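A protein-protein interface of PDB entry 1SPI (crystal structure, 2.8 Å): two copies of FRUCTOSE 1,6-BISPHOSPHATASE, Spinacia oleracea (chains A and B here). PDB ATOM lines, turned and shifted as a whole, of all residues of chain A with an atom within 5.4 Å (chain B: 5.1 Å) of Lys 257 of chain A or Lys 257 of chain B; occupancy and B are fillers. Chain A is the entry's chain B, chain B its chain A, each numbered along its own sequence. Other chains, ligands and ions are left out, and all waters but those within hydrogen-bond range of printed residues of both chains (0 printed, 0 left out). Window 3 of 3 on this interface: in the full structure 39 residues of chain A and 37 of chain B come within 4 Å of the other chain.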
ATOM      1  N   TYR A 235      14.303 -17.008  -7.826  1.00  0.00           N
ATOM      2  CA  TYR A 235      14.690 -15.667  -8.263  1.00  0.00           C
ATOM      3  C   TYR A 235      14.127 -14.617  -7.333  1.00  0.00           C
ATOM      4  O   TYR A 235      13.037 -14.805  -6.776  1.00  0.00           O
ATOM      5  CB  TYR A 235      14.302 -15.384  -9.731  1.00  0.00           C
ATOM      6  CG  TYR A 235      12.839 -15.262  -9.950  1.00  0.00           C
ATOM      7  CD1 TYR A 235      12.063 -16.386 -10.110  1.00  0.00           C
ATOM      8  CD2 TYR A 235      12.211 -14.031  -9.935  1.00  0.00           C
ATOM      9  CE1 TYR A 235      10.673 -16.293 -10.244  1.00  0.00           C
ATOM     10  CE2 TYR A 235      10.819 -13.925 -10.065  1.00  0.00           C
ATOM     11  CZ  TYR A 235      10.064 -15.063 -10.213  1.00  0.00           C
ATOM     12  OH  TYR A 235       8.703 -15.041 -10.244  1.00  0.00           O
ATOM     13  N   GLU A 239       9.676  -7.851  -8.937  1.00  0.00           N
ATOM     14  CA  GLU A 239       8.768  -7.989 -10.083  1.00  0.00           C
ATOM     15  C   GLU A 239       7.741  -6.869 -10.221  1.00  0.00           C
ATOM     16  O   GLU A 239       7.386  -6.467 -11.337  1.00  0.00           O
ATOM     17  CB  GLU A 239       8.077  -9.353 -10.064  1.00  0.00           C
ATOM     18  CG  GLU A 239       9.095 -10.505 -10.065  1.00  0.00           C
ATOM     19  CD  GLU A 239       8.483 -11.919 -10.088  1.00  0.00           C
ATOM     20  OE1 GLU A 239       7.962 -12.334 -11.151  1.00  0.00           O
ATOM     21  OE2 GLU A 239       8.589 -12.635  -9.057  1.00  0.00           O
ATOM     22  N   GLY A 240       7.419  -6.251  -9.092  1.00  0.00           N
ATOM     23  CA  GLY A 240       6.412  -5.190  -9.082  1.00  0.00           C
ATOM     24  C   GLY A 240       6.641  -3.960  -9.943  1.00  0.00           C
ATOM     25  O   GLY A 240       5.740  -3.117 -10.117  1.00  0.00           O
ATOM     26  N   TYR A 242       8.132  -4.265 -13.039  1.00  0.00           N
ATOM     27  CA  TYR A 242       8.498  -4.987 -14.270  1.00  0.00           C
ATOM     28  C   TYR A 242       8.211  -4.113 -15.478  1.00  0.00           C
ATOM     29  O   TYR A 242       9.007  -4.075 -16.417  1.00  0.00           O
ATOM     30  CB  TYR A 242       7.657  -6.258 -14.376  1.00  0.00           C
ATOM     31  CG  TYR A 242       7.385  -6.821 -15.769  1.00  0.00           C
ATOM     32  CD1 TYR A 242       6.450  -6.225 -16.629  1.00  0.00           C
ATOM     33  CD2 TYR A 242       7.949  -8.036 -16.159  1.00  0.00           C
ATOM     34  CE1 TYR A 242       6.086  -6.851 -17.848  1.00  0.00           C
ATOM     35  CE2 TYR A 242       7.600  -8.654 -17.350  1.00  0.00           C
ATOM     36  CZ  TYR A 242       6.678  -8.076 -18.192  1.00  0.00           C
ATOM     37  OH  TYR A 242       6.383  -8.719 -19.378  1.00  0.00           O
ATOM     38  N   LYS A 243       7.038  -3.473 -15.465  1.00  0.00           N
ATOM     39  CA  LYS A 243       6.590  -2.576 -16.523  1.00  0.00           C
ATOM     40  C   LYS A 243       7.410  -1.296 -16.525  1.00  0.00           C
ATOM     41  O   LYS A 243       6.879  -0.225 -16.805  1.00  0.00           O
ATOM     42  CB  LYS A 243       5.130  -2.197 -16.297  1.00  0.00           C
ATOM     43  CG  LYS A 243       4.405  -1.747 -17.566  1.00  0.00           C
ATOM     44  CD  LYS A 243       3.608  -0.448 -17.371  1.00  0.00           C
ATOM     45  CE  LYS A 243       2.095  -0.726 -17.399  1.00  0.00           C
ATOM     46  NZ  LYS A 243       1.597  -1.087 -18.751  1.00  0.00           N
ATOM     47  N   MET A 253      11.972 -11.944 -17.572  1.00  0.00           N
ATOM     48  CA  MET A 253      10.994 -12.204 -16.534  1.00  0.00           C
ATOM     49  C   MET A 253       9.967 -13.226 -16.935  1.00  0.00           C
ATOM     50  O   MET A 253       9.685 -14.121 -16.144  1.00  0.00           O
ATOM     51  CB  MET A 253      10.277 -10.960 -16.069  1.00  0.00           C
ATOM     52  CG  MET A 253      11.118  -9.704 -16.114  1.00  0.00           C
ATOM     53  SD  MET A 253      12.712  -9.931 -15.243  1.00  0.00           S
ATOM     54  CE  MET A 253      12.044 -10.538 -13.539  1.00  0.00           C
ATOM     55  N   ASP A 254       9.544 -13.227 -18.201  1.00  0.00           N
ATOM     56  CA  ASP A 254       8.509 -14.172 -18.626  1.00  0.00           C
ATOM     57  C   ASP A 254       8.957 -15.598 -18.802  1.00  0.00           C
ATOM     58  O   ASP A 254       8.194 -16.513 -18.506  1.00  0.00           O
ATOM     59  CB  ASP A 254       7.734 -13.705 -19.859  1.00  0.00           C
ATOM     60  CG  ASP A 254       6.452 -14.513 -20.068  1.00  0.00           C
ATOM     61  OD1 ASP A 254       6.558 -15.665 -20.587  1.00  0.00           O
ATOM     62  OD2 ASP A 254       5.328 -14.033 -19.689  1.00  0.00           O
ATOM     63  N   ASP A 255      10.204 -15.815 -19.192  1.00  0.00           N
ATOM     64  CA  ASP A 255      10.694 -17.191 -19.355  1.00  0.00           C
ATOM     65  C   ASP A 255      11.095 -17.860 -18.013  1.00  0.00           C
ATOM     66  O   ASP A 255      11.781 -18.889 -17.964  1.00  0.00           O
ATOM     67  CB  ASP A 255      11.800 -17.218 -20.396  1.00  0.00           C
ATOM     68  CG  ASP A 255      11.519 -16.250 -21.555  1.00  0.00           C
ATOM     69  OD1 ASP A 255      10.651 -16.565 -22.421  1.00  0.00           O
ATOM     70  OD2 ASP A 255      12.138 -15.152 -21.544  1.00  0.00           O
ATOM     71  N   LEU A 256      10.675 -17.224 -16.921  1.00  0.00           N
ATOM     72  CA  LEU A 256      10.871 -17.690 -15.546  1.00  0.00           C
ATOM     73  C   LEU A 256       9.468 -18.154 -15.166  1.00  0.00           C
ATOM     74  O   LEU A 256       9.303 -19.103 -14.402  1.00  0.00           O
ATOM     75  CB  LEU A 256      11.226 -16.512 -14.654  1.00  0.00           C
ATOM     76  CG  LEU A 256      12.630 -16.381 -14.097  1.00  0.00           C
ATOM     77  CD1 LEU A 256      13.682 -17.246 -14.795  1.00  0.00           C
ATOM     78  CD2 LEU A 256      12.985 -14.907 -14.188  1.00  0.00           C
ATOM     79  N   LYS A 257       8.456 -17.435 -15.658  1.00  0.00           N
ATOM     80  CA  LYS A 257       7.073 -17.774 -15.402  1.00  0.00           C
ATOM     81  C   LYS A 257       6.608 -18.883 -16.344  1.00  0.00           C
ATOM     82  O   LYS A 257       5.954 -19.850 -15.912  1.00  0.00           O
ATOM     83  CB  LYS A 257       6.177 -16.572 -15.656  1.00  0.00           C
ATOM     84  CG  LYS A 257       6.146 -15.581 -14.567  1.00  0.00           C
ATOM     85  CD  LYS A 257       5.137 -14.519 -14.864  1.00  0.00           C
ATOM     86  CE  LYS A 257       5.161 -13.484 -13.765  1.00  0.00           C
ATOM     87  NZ  LYS A 257       4.202 -12.359 -14.005  1.00  0.00           N
ATOM     88  N   GLU A 258       6.999 -18.756 -17.620  1.00  0.00           N
ATOM     89  CA  GLU A 258       6.570 -19.652 -18.710  1.00  0.00           C
ATOM     90  C   GLU A 258       7.551 -20.671 -19.274  1.00  0.00           C
ATOM     91  O   GLU A 258       8.043 -20.512 -20.392  1.00  0.00           O
ATOM     92  CB  GLU A 258       6.070 -18.811 -19.866  1.00  0.00           C
ATOM     93  CG  GLU A 258       4.578 -18.776 -20.011  1.00  0.00           C
ATOM     94  CD  GLU A 258       3.937 -17.794 -19.077  1.00  0.00           C
ATOM     95  OE1 GLU A 258       4.161 -16.567 -19.284  1.00  0.00           O
ATOM     96  OE2 GLU A 258       3.193 -18.255 -18.168  1.00  0.00           O
ATOM     97  N   PRO A 259       7.781 -21.768 -18.549  1.00  0.00           N
ATOM     98  CA  PRO A 259       8.685 -22.861 -18.917  1.00  0.00           C
ATOM     99  C   PRO A 259       8.599 -23.233 -20.402  1.00  0.00           C
ATOM    100  O   PRO A 259       7.738 -22.740 -21.109  1.00  0.00           O
ATOM    101  CB  PRO A 259       8.182 -24.004 -18.036  1.00  0.00           C
ATOM    102  CG  PRO A 259       7.828 -23.279 -16.757  1.00  0.00           C
ATOM    103  CD  PRO A 259       7.105 -22.058 -17.269  1.00  0.00           C
ATOM    104  N   TYR B 235       1.907  -6.399  -2.988  1.00  0.00           N
ATOM    105  CA  TYR B 235       1.256  -7.644  -3.355  1.00  0.00           C
ATOM    106  C   TYR B 235       2.176  -8.818  -3.114  1.00  0.00           C
ATOM    107  O   TYR B 235       3.364  -8.806  -3.527  1.00  0.00           O
ATOM    108  CB  TYR B 235       0.681  -7.575  -4.782  1.00  0.00           C
ATOM    109  CG  TYR B 235       1.595  -7.949  -5.939  1.00  0.00           C
ATOM    110  CD1 TYR B 235       1.780  -9.280  -6.292  1.00  0.00           C
ATOM    111  CD2 TYR B 235       2.252  -6.969  -6.730  1.00  0.00           C
ATOM    112  CE1 TYR B 235       2.567  -9.634  -7.368  1.00  0.00           C
ATOM    113  CE2 TYR B 235       3.053  -7.340  -7.822  1.00  0.00           C
ATOM    114  CZ  TYR B 235       3.192  -8.681  -8.121  1.00  0.00           C
ATOM    115  OH  TYR B 235       3.941  -9.144  -9.170  1.00  0.00           O
ATOM    116  N   GLU B 239       4.395 -15.797  -7.649  1.00  0.00           N
ATOM    117  CA  GLU B 239       4.321 -15.846  -9.100  1.00  0.00           C
ATOM    118  C   GLU B 239       5.043 -17.050  -9.715  1.00  0.00           C
ATOM    119  O   GLU B 239       4.594 -17.565 -10.739  1.00  0.00           O
ATOM    120  CB  GLU B 239       4.845 -14.548  -9.705  1.00  0.00           C
ATOM    121  CG  GLU B 239       4.207 -13.331  -9.138  1.00  0.00           C
ATOM    122  CD  GLU B 239       4.097 -12.247 -10.157  1.00  0.00           C
ATOM    123  OE1 GLU B 239       5.055 -11.491 -10.367  1.00  0.00           O
ATOM    124  OE2 GLU B 239       3.041 -12.159 -10.791  1.00  0.00           O
ATOM    125  N   GLY B 240       6.080 -17.561  -9.055  1.00  0.00           N
ATOM    126  CA  GLY B 240       6.850 -18.680  -9.590  1.00  0.00           C
ATOM    127  C   GLY B 240       6.108 -19.823 -10.255  1.00  0.00           C
ATOM    128  O   GLY B 240       6.635 -20.490 -11.139  1.00  0.00           O
ATOM    129  N   TYR B 242       3.194 -19.418 -11.766  1.00  0.00           N
ATOM    130  CA  TYR B 242       2.206 -18.638 -12.529  1.00  0.00           C
ATOM    131  C   TYR B 242       1.458 -19.430 -13.619  1.00  0.00           C
ATOM    132  O   TYR B 242       0.243 -19.345 -13.725  1.00  0.00           O
ATOM    133  CB  TYR B 242       2.907 -17.470 -13.192  1.00  0.00           C
ATOM    134  CG  TYR B 242       2.007 -16.411 -13.742  1.00  0.00           C
ATOM    135  CD1 TYR B 242       1.656 -15.332 -12.943  1.00  0.00           C
ATOM    136  CD2 TYR B 242       1.618 -16.411 -15.073  1.00  0.00           C
ATOM    137  CE1 TYR B 242       0.952 -14.276 -13.442  1.00  0.00           C
ATOM    138  CE2 TYR B 242       0.926 -15.351 -15.597  1.00  0.00           C
ATOM    139  CZ  TYR B 242       0.580 -14.264 -14.768  1.00  0.00           C
ATOM    140  OH  TYR B 242      -0.153 -13.156 -15.198  1.00  0.00           O
ATOM    141  N   LYS B 243       2.207 -20.177 -14.422  1.00  0.00           N
ATOM    142  CA  LYS B 243       1.669 -21.003 -15.505  1.00  0.00           C
ATOM    143  C   LYS B 243       0.860 -22.181 -14.876  1.00  0.00           C
ATOM    144  O   LYS B 243       0.936 -23.342 -15.305  1.00  0.00           O
ATOM    145  CB  LYS B 243       2.859 -21.504 -16.339  1.00  0.00           C
ATOM    146  CG  LYS B 243       2.553 -22.535 -17.396  1.00  0.00           C
ATOM    147  CD  LYS B 243       3.746 -23.443 -17.580  1.00  0.00           C
ATOM    148  CE  LYS B 243       4.222 -23.950 -16.237  1.00  0.00           C
ATOM    149  NZ  LYS B 243       3.084 -24.643 -15.587  1.00  0.00           N
ATOM    150  N   MET B 253      -2.858 -11.086 -11.392  1.00  0.00           N
ATOM    151  CA  MET B 253      -1.407 -10.919 -11.371  1.00  0.00           C
ATOM    152  C   MET B 253      -0.859  -9.969 -12.456  1.00  0.00           C
ATOM    153  O   MET B 253      -0.800  -8.777 -12.203  1.00  0.00           O
ATOM    154  CB  MET B 253      -0.708 -12.283 -11.355  1.00  0.00           C
ATOM    155  CG  MET B 253      -1.455 -13.306 -10.520  1.00  0.00           C
ATOM    156  SD  MET B 253      -1.230 -13.142  -8.737  1.00  0.00           S
ATOM    157  CE  MET B 253      -1.158 -11.290  -8.431  1.00  0.00           C
ATOM    158  N   ASP B 254      -0.700 -10.431 -13.700  1.00  0.00           N
ATOM    159  CA  ASP B 254      -0.121  -9.601 -14.767  1.00  0.00           C
ATOM    160  C   ASP B 254      -0.676  -8.174 -14.914  1.00  0.00           C
ATOM    161  O   ASP B 254       0.029  -7.279 -15.352  1.00  0.00           O
ATOM    162  CB  ASP B 254      -0.134 -10.344 -16.111  1.00  0.00           C
ATOM    163  CG  ASP B 254      -1.549 -10.694 -16.597  1.00  0.00           C
ATOM    164  OD1 ASP B 254      -2.539 -10.085 -16.107  1.00  0.00           O
ATOM    165  OD2 ASP B 254      -1.679 -11.577 -17.495  1.00  0.00           O
ATOM    166  N   ASP B 255      -1.892  -7.942 -14.446  1.00  0.00           N
ATOM    167  CA  ASP B 255      -2.508  -6.634 -14.527  1.00  0.00           C
ATOM    168  C   ASP B 255      -2.176  -5.666 -13.380  1.00  0.00           C
ATOM    169  O   ASP B 255      -2.012  -4.486 -13.653  1.00  0.00           O
ATOM    170  CB  ASP B 255      -4.011  -6.808 -14.683  1.00  0.00           C
ATOM    171  CG  ASP B 255      -4.775  -5.514 -14.569  1.00  0.00           C
ATOM    172  OD1 ASP B 255      -4.222  -4.462 -14.913  1.00  0.00           O
ATOM    173  OD2 ASP B 255      -5.948  -5.557 -14.130  1.00  0.00           O
ATOM    174  N   LEU B 256      -2.044  -6.111 -12.123  1.00  0.00           N
ATOM    175  CA  LEU B 256      -1.721  -5.147 -11.023  1.00  0.00           C
ATOM    176  C   LEU B 256      -0.343  -4.463 -11.077  1.00  0.00           C
ATOM    177  O   LEU B 256      -0.145  -3.425 -10.423  1.00  0.00           O
ATOM    178  CB  LEU B 256      -1.919  -5.754  -9.618  1.00  0.00           C
ATOM    179  CG  LEU B 256      -0.850  -6.545  -8.864  1.00  0.00           C
ATOM    180  CD1 LEU B 256      -1.408  -6.981  -7.522  1.00  0.00           C
ATOM    181  CD2 LEU B 256      -0.466  -7.759  -9.629  1.00  0.00           C
ATOM    182  N   LYS B 257       0.580  -5.058 -11.844  1.00  0.00           N
ATOM    183  CA  LYS B 257       1.931  -4.547 -12.034  1.00  0.00           C
ATOM    184  C   LYS B 257       1.982  -3.657 -13.296  1.00  0.00           C
ATOM    185  O   LYS B 257       3.080  -3.286 -13.733  1.00  0.00           O
ATOM    186  CB  LYS B 257       2.924  -5.699 -12.176  1.00  0.00           C
ATOM    187  CG  LYS B 257       2.903  -6.346 -13.528  1.00  0.00           C
ATOM    188  CD  LYS B 257       3.432  -7.777 -13.459  1.00  0.00           C
ATOM    189  CE  LYS B 257       2.639  -8.614 -12.446  1.00  0.00           C
ATOM    190  NZ  LYS B 257       2.433 -10.104 -12.718  1.00  0.00           N
ATOM    191  N   GLU B 258       0.812  -3.371 -13.900  1.00  0.00           N
ATOM    192  CA  GLU B 258       0.701  -2.487 -15.085  1.00  0.00           C
ATOM    193  C   GLU B 258      -0.187  -1.364 -14.545  1.00  0.00           C
ATOM    194  O   GLU B 258      -1.340  -1.302 -14.879  1.00  0.00           O
ATOM    195  CB  GLU B 258      -0.069  -3.154 -16.278  1.00  0.00           C
ATOM    196  CG  GLU B 258       0.361  -4.592 -16.754  1.00  0.00           C
ATOM    197  CD  GLU B 258       1.504  -4.617 -17.759  1.00  0.00           C
ATOM    198  OE1 GLU B 258       1.732  -3.584 -18.437  1.00  0.00           O
ATOM    199  OE2 GLU B 258       2.176  -5.677 -17.852  1.00  0.00           O
ATOM    200  N   PRO B 259       0.365  -0.422 -13.772  1.00  0.00           N
ATOM    201  CA  PRO B 259      -0.478   0.662 -13.221  1.00  0.00           C
ATOM    202  C   PRO B 259      -1.669   1.161 -14.079  1.00  0.00           C
ATOM    203  O   PRO B 259      -2.826   0.911 -13.745  1.00  0.00           O
ATOM    204  CB  PRO B 259       0.548   1.773 -12.884  1.00  0.00           C
ATOM    205  CG  PRO B 259       1.742   0.966 -12.437  1.00  0.00           C
ATOM    206  CD  PRO B 259       1.791  -0.136 -13.535  1.00  0.00           C
ATOM    207  N   PRO B 265       3.450   1.445  -8.698  1.00  0.00           N
ATOM    208  CA  PRO B 265       2.917   0.118  -9.051  1.00  0.00           C
ATOM    209  C   PRO B 265       2.900  -0.644  -7.744  1.00  0.00           C
ATOM    210  O   PRO B 265       3.536  -0.228  -6.773  1.00  0.00           O
ATOM    211  CB  PRO B 265       4.009  -0.489  -9.934  1.00  0.00           C
ATOM    212  CG  PRO B 265       5.271   0.089  -9.320  1.00  0.00           C
ATOM    213  CD  PRO B 265       4.871   1.563  -9.059  1.00  0.00           C
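OE1 of Glu 239 of chain B sits close to OE1 of Glu 239 of chain A (3.1 Å). The side-chain amino group (NZ) of Lys 257 of chain A sits close to the side-chain amino group (NZ) of Lys 257 of chain B (3.1 Å). The side-chain carboxylate (OE1) of Glu 258 of chain B lies within salt-bridge range of the side-chain amino group (NZ) of Lys 243 of chain A, 2.5 Å away. OE2 of Glu 239 of chain B is in salt-bridge range of NZ of Lys 257 of chain A (3.4 Å).
OH of Tyr 235 of chain B lies within hydrogen-bond range of OE1 of Glu 239 of chain B (2.9 Å). OH of Tyr 235 of chain A sits at hydrogen-bond distance from OE2 of Glu 239 of chain A, 2.7 Å away. The side-chain amino group (NZ) of Lys 257 of chain B lies within salt-bridge range of the side-chain carboxylate (OE2) of Glu 239 of chain B (2.9 Å). The side-chain hydroxyl of Tyr 242 of chain B lies close to the backbone NH of Asp 254 of chain B.
Among the printed residues, merely in contact across the chains: Gly 240 of chain A with Pro 265 of chain B (3.2 Å), Lys 243 of chain A with Lys 257 of chain B (3.5 Å), Lys 257 of chain A with Lys 243 of chain B (3.5 Å), Pro 259 of chain A with Lys 243 of chain B (3.6 Å), Glu 258 of chain A with Lys 243 of chain B (3.7 Å), Lys 257 of chain A with Tyr 242 of chain B (3.8 Å), Tyr 235 of chain A with Gly 240 of chain B (3.8 Å), Lys 243 of chain A with Pro 259 of chain B (3.9 Å), Tyr 235 of chain A with Glu 239 of chain B (3.9 Å) and Glu 258 of chain A with Tyr 242 of chain B (3.9 Å).
Of the printed residues of chain A, Lys 257 of chain B touches Lys 243 and Lys 257. Printed residues of chain B within 4 Å of Glu 239 of chain A: Glu 239 (3.1 Å). Of the printed residues of chain B, Pro 259 of chain A touches Lys 243 (3.6 Å). Of the printed residues of chain B, Tyr 235 of chain A touches Glu 239 (3.9 Å) and Gly 240 (3.8 Å). Printed residues of chain B within 4 Å of Lys 243 of chain A: Lys 257 (3.5 Å), Glu 258 (2.5 Å) and Pro 259 (3.9 Å). Tyr 242 of chain A touches none of the printed residues of chain B. The nearest residue of chain A that does not touch Lys 257 of chain B is Gly 240 of chain A (4.3 Å). The nearest printed residue of chain A that does not touch Pro 265 of chain B is Tyr 242 of chain A (6.4 Å).
Printed residues of chain A that touch a printed residue of chain B: Tyr 235, Glu 239, Gly 240, Lys 243, Lys 257, Glu 258 and Pro 259. Hydrophobic or aromatic side chains of chain A that line the printed part of chain B: Tyr 235 and Pro 259. Of the 13 printed residues of chain B, 8 touch a printed residue of chain A. Among the printed residues, 14 pairs touch across the chains. Among the printed residues, Asp or Glu carboxylates within 4 Å of a Lys or Arg side-chain nitrogen of the other chain: Lys 243 of chain A with Glu 258 of chain B and Lys 257 of chain A with Glu 239 of chain B.
Tyr 235 of chain A touches Glu 239 of chain B, but with the chains exchanged Glu 239 of chain A does not touch Tyr 235 of chain B (4.2 Å). Tyr 235 of chain A touches Gly 240 of chain B, but with the chains exchanged Gly 240 of chain A does not touch Tyr 235 of chain B (4.2 Å). Lys 243 of chain A touches Pro 259 of chain B, and with the chains exchanged Pro 259 of chain A touches Lys 243 of chain B. Lys 257 of chain A touches Tyr 242 of chain B, but with the chains exchanged Tyr 242 of chain A does not touch Lys 257 of chain B (4.6 Å). Positions printed for both chains: 235, 239, 240, 242, 243, 253, 254, 255, 256, 257, 258 and 259.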
